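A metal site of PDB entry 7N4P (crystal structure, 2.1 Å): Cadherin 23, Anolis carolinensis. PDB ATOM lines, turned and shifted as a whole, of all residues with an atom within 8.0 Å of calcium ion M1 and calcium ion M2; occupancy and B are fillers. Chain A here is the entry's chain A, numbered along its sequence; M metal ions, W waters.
Calcium ion M1 is bound by the backbone carbonyl oxygen of Val 205 (2.3 Å), water W3 (2.3 Å), water W2 (2.3 Å), the side-chain carboxylate of Asp 204 (2.4 Å), the side-chain carboxylate of Glu 119 (2.5 Å) and the side-chain carboxylate of Glu 172 (2.6 Å). Calcium ion M1 has six donor atoms within binding distance. Slightly farther from calcium ion M1 lies the side-chain carboxylate (OE1) of Glu 172 (2.9 Å).
OE1 of Glu 119 sits close to N of Tyr 171 (3.2 Å). O of Thr 203 sits at hydrogen-bond distance from N of Glu 119 (3.1 Å).
Within 4 Å of calcium ion M1: Glu 119, Glu 172, Asp 204 and Val 205. The nearest printed residue that does not touch calcium ion M1 is Asp 207 (4.05 Å).
Calcium ion M2 is bound by water W1. Calcium ion M2 is bound by water W4. Calcium ion M2 is bound by OE1 of Glu 119 (2.4 Å). OE1 of Glu 172 binds calcium ion M2, at 2.4 Å. The side-chain carboxylate (OD1) of Asp 170 is bound to calcium ion M2 (2.6 Å). Calcium ion M2 has five donor atoms within binding distance. Slightly farther from calcium ion M2 lies water W2 (3.1 Å).
Within 4 Å of calcium ion M2: Glu 119, Asp 170 and Glu 172.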
ATOM      1  N   GLU A 119       2.842   5.391 -16.984  1.00  0.00           N
ATOM      2  CA  GLU A 119       2.506   3.942 -16.929  1.00  0.00           C
ATOM      3  C   GLU A 119       1.005   3.753 -17.043  1.00  0.00           C
ATOM      4  O   GLU A 119       0.651   2.681 -17.425  1.00  0.00           O
ATOM      5  CB  GLU A 119       2.984   3.247 -15.657  1.00  0.00           C
ATOM      6  CG  GLU A 119       2.386   3.835 -14.392  1.00  0.00           C
ATOM      7  CD  GLU A 119       2.785   3.105 -13.123  1.00  0.00           C
ATOM      8  OE1 GLU A 119       2.722   1.877 -13.105  1.00  0.00           O
ATOM      9  OE2 GLU A 119       3.135   3.772 -12.179  1.00  0.00           O
ATOM     10  N   ASN A 120       0.185   4.739 -16.643  1.00  0.00           N
ATOM     11  CA  ASN A 120      -1.300   4.672 -16.670  1.00  0.00           C
ATOM     12  C   ASN A 120      -1.839   5.204 -18.000  1.00  0.00           C
ATOM     13  O   ASN A 120      -3.008   5.566 -18.020  1.00  0.00           O
ATOM     14  CB  ASN A 120      -1.947   5.414 -15.497  1.00  0.00           C
ATOM     15  CG  ASN A 120      -1.781   6.929 -15.510  1.00  0.00           C
ATOM     16  OD1 ASN A 120      -0.953   7.530 -16.183  1.00  0.00           O
ATOM     17  ND2 ASN A 120      -2.631   7.598 -14.779  1.00  0.00           N
ATOM     18  N   LEU A 169       0.456  -0.707 -19.356  1.00  0.00           N
ATOM     19  CA  LEU A 169       1.870  -0.617 -18.942  1.00  0.00           C
ATOM     20  C   LEU A 169       2.009  -0.753 -17.393  1.00  0.00           C
ATOM     21  O   LEU A 169       1.008  -0.716 -16.688  1.00  0.00           O
ATOM     22  CB  LEU A 169       2.328   0.753 -19.455  1.00  0.00           C
ATOM     23  CG  LEU A 169       2.179   0.920 -20.961  1.00  0.00           C
ATOM     24  CD1 LEU A 169       2.537   2.331 -21.359  1.00  0.00           C
ATOM     25  CD2 LEU A 169       3.051  -0.087 -21.689  1.00  0.00           C
ATOM     26  N   ASP A 170       3.234  -0.840 -16.898  1.00  0.00           N
ATOM     27  CA  ASP A 170       3.544  -1.046 -15.473  1.00  0.00           C
ATOM     28  C   ASP A 170       4.991  -0.647 -15.232  1.00  0.00           C
ATOM     29  O   ASP A 170       5.874  -1.515 -15.513  1.00  0.00           O
ATOM     30  CB  ASP A 170       3.329  -2.495 -15.065  1.00  0.00           C
ATOM     31  CG  ASP A 170       3.264  -2.675 -13.556  1.00  0.00           C
ATOM     32  OD1 ASP A 170       3.666  -1.721 -12.808  1.00  0.00           O
ATOM     33  OD2 ASP A 170       2.796  -3.743 -13.173  1.00  0.00           O
ATOM     34  N   TYR A 171       5.177   0.566 -14.686  1.00  0.00           N
ATOM     35  CA  TYR A 171       6.493   1.164 -14.324  1.00  0.00           C
ATOM     36  C   TYR A 171       7.283   0.175 -13.479  1.00  0.00           C
ATOM     37  O   TYR A 171       8.503   0.136 -13.630  1.00  0.00           O
ATOM     38  CB  TYR A 171       6.339   2.470 -13.541  1.00  0.00           C
ATOM     39  CG  TYR A 171       7.661   3.089 -13.161  1.00  0.00           C
ATOM     40  CD1 TYR A 171       8.318   3.944 -14.035  1.00  0.00           C
ATOM     41  CD2 TYR A 171       8.247   2.840 -11.913  1.00  0.00           C
ATOM     42  CE1 TYR A 171       9.521   4.527 -13.687  1.00  0.00           C
ATOM     43  CE2 TYR A 171       9.456   3.420 -11.553  1.00  0.00           C
ATOM     44  CZ  TYR A 171      10.099   4.259 -12.448  1.00  0.00           C
ATOM     45  OH  TYR A 171      11.283   4.818 -12.121  1.00  0.00           O
ATOM     46  N   GLU A 172       6.574  -0.557 -12.597  1.00  0.00           N
ATOM     47  CA  GLU A 172       7.153  -1.497 -11.613  1.00  0.00           C
ATOM     48  C   GLU A 172       7.721  -2.720 -12.343  1.00  0.00           C
ATOM     49  O   GLU A 172       8.683  -3.290 -11.856  1.00  0.00           O
ATOM     50  CB  GLU A 172       6.121  -1.903 -10.543  1.00  0.00           C
ATOM     51  CG  GLU A 172       5.934  -0.878  -9.426  1.00  0.00           C
ATOM     52  CD  GLU A 172       5.111   0.383  -9.754  1.00  0.00           C
ATOM     53  OE1 GLU A 172       4.169   0.301 -10.589  1.00  0.00           O
ATOM     54  OE2 GLU A 172       5.387   1.452  -9.150  1.00  0.00           O
ATOM     55  N   VAL A 173       7.184  -3.065 -13.504  1.00  0.00           N
ATOM     56  CA  VAL A 173       7.704  -4.204 -14.303  1.00  0.00           C
ATOM     57  C   VAL A 173       8.707  -3.675 -15.328  1.00  0.00           C
ATOM     58  O   VAL A 173       9.770  -4.282 -15.447  1.00  0.00           O
ATOM     59  CB  VAL A 173       6.565  -5.000 -14.952  1.00  0.00           C
ATOM     60  CG1 VAL A 173       7.094  -5.957 -16.000  1.00  0.00           C
ATOM     61  CG2 VAL A 173       5.771  -5.756 -13.899  1.00  0.00           C
ATOM     62  N   ILE A 202       8.897   5.186 -19.495  1.00  0.00           N
ATOM     63  CA  ILE A 202       7.654   5.044 -18.700  1.00  0.00           C
ATOM     64  C   ILE A 202       7.892   5.826 -17.407  1.00  0.00           C
ATOM     65  O   ILE A 202       8.966   5.613 -16.790  1.00  0.00           O
ATOM     66  CB  ILE A 202       7.325   3.563 -18.470  1.00  0.00           C
ATOM     67  CG1 ILE A 202       7.397   2.783 -19.784  1.00  0.00           C
ATOM     68  CG2 ILE A 202       5.990   3.390 -17.776  1.00  0.00           C
ATOM     69  CD1 ILE A 202       6.251   3.093 -20.770  1.00  0.00           C
ATOM     70  N   THR A 203       6.990   6.753 -17.078  1.00  0.00           N
ATOM     71  CA  THR A 203       6.988   7.536 -15.821  1.00  0.00           C
ATOM     72  C   THR A 203       6.131   6.817 -14.769  1.00  0.00           C
ATOM     73  O   THR A 203       5.060   6.286 -15.064  1.00  0.00           O
ATOM     74  CB  THR A 203       6.593   9.001 -16.074  1.00  0.00           C
ATOM     75  OG1 THR A 203       5.317   9.018 -16.714  1.00  0.00           O
ATOM     76  CG2 THR A 203       7.586   9.728 -16.950  1.00  0.00           C
ATOM     77  N   ASP A 204       6.648   6.747 -13.548  1.00  0.00           N
ATOM     78  CA  ASP A 204       5.940   6.130 -12.405  1.00  0.00           C
ATOM     79  C   ASP A 204       4.737   7.004 -12.024  1.00  0.00           C
ATOM     80  O   ASP A 204       4.861   8.221 -11.994  1.00  0.00           O
ATOM     81  CB  ASP A 204       6.896   5.973 -11.242  1.00  0.00           C
ATOM     82  CG  ASP A 204       6.297   5.317 -10.025  1.00  0.00           C
ATOM     83  OD1 ASP A 204       5.311   4.582 -10.138  1.00  0.00           O
ATOM     84  OD2 ASP A 204       6.834   5.577  -8.974  1.00  0.00           O
ATOM     85  N   VAL A 205       3.621   6.362 -11.704  1.00  0.00           N
ATOM     86  CA  VAL A 205       2.393   6.957 -11.122  1.00  0.00           C
ATOM     87  C   VAL A 205       2.079   6.195  -9.829  1.00  0.00           C
ATOM     88  O   VAL A 205       2.179   4.939  -9.840  1.00  0.00           O
ATOM     89  CB  VAL A 205       1.237   6.796 -12.130  1.00  0.00           C
ATOM     90  CG1 VAL A 205      -0.113   6.922 -11.451  1.00  0.00           C
ATOM     91  CG2 VAL A 205       1.390   7.751 -13.298  1.00  0.00           C
ATOM     92  N   GLN A 206       1.654   6.904  -8.795  1.00  0.00           N
ATOM     93  CA  GLN A 206       1.241   6.305  -7.502  1.00  0.00           C
ATOM     94  C   GLN A 206      -0.041   5.518  -7.717  1.00  0.00           C
ATOM     95  O   GLN A 206      -0.956   6.116  -8.292  1.00  0.00           O
ATOM     96  CB  GLN A 206       0.954   7.408  -6.495  1.00  0.00           C
ATOM     97  CG  GLN A 206       2.178   8.223  -6.132  1.00  0.00           C
ATOM     98  CD  GLN A 206       1.932   9.168  -4.982  1.00  0.00           C
ATOM     99  OE1 GLN A 206       0.833   9.291  -4.442  1.00  0.00           O
ATOM    100  NE2 GLN A 206       2.976   9.882  -4.581  1.00  0.00           N
ATOM    101  N   ASP A 207      -0.110   4.252  -7.287  1.00  0.00           N
ATOM    102  CA  ASP A 207      -1.366   3.437  -7.271  1.00  0.00           C
ATOM    103  C   ASP A 207      -1.888   3.302  -5.827  1.00  0.00           C
ATOM    104  O   ASP A 207      -2.571   4.189  -5.325  1.00  0.00           O
ATOM    105  CB  ASP A 207      -1.163   2.049  -7.913  1.00  0.00           C
ATOM    106  CG  ASP A 207      -0.116   1.181  -7.227  1.00  0.00           C
ATOM    107  OD1 ASP A 207      -0.168   1.065  -5.966  1.00  0.00           O
ATOM    108  OD2 ASP A 207       0.776   0.650  -7.952  1.00  0.00           O
HETATM  109 CA    CA M   1       3.460   3.049  -9.801  1.00  0.00          CA
HETATM  110 CA    CA M   2       2.091   0.087 -11.702  1.00  0.00          CA
HETATM  111  O   HOH W   1       1.314  -1.126 -10.197  1.00  0.00           O
HETATM  112  O   HOH W   2       1.189   2.489  -9.906  1.00  0.00           O
HETATM  113  O   HOH W   3       2.997   3.732  -7.644  1.00  0.00           O
HETATM  114  O   HOH W   4       0.510  -0.687 -13.097  1.00  0.00           O
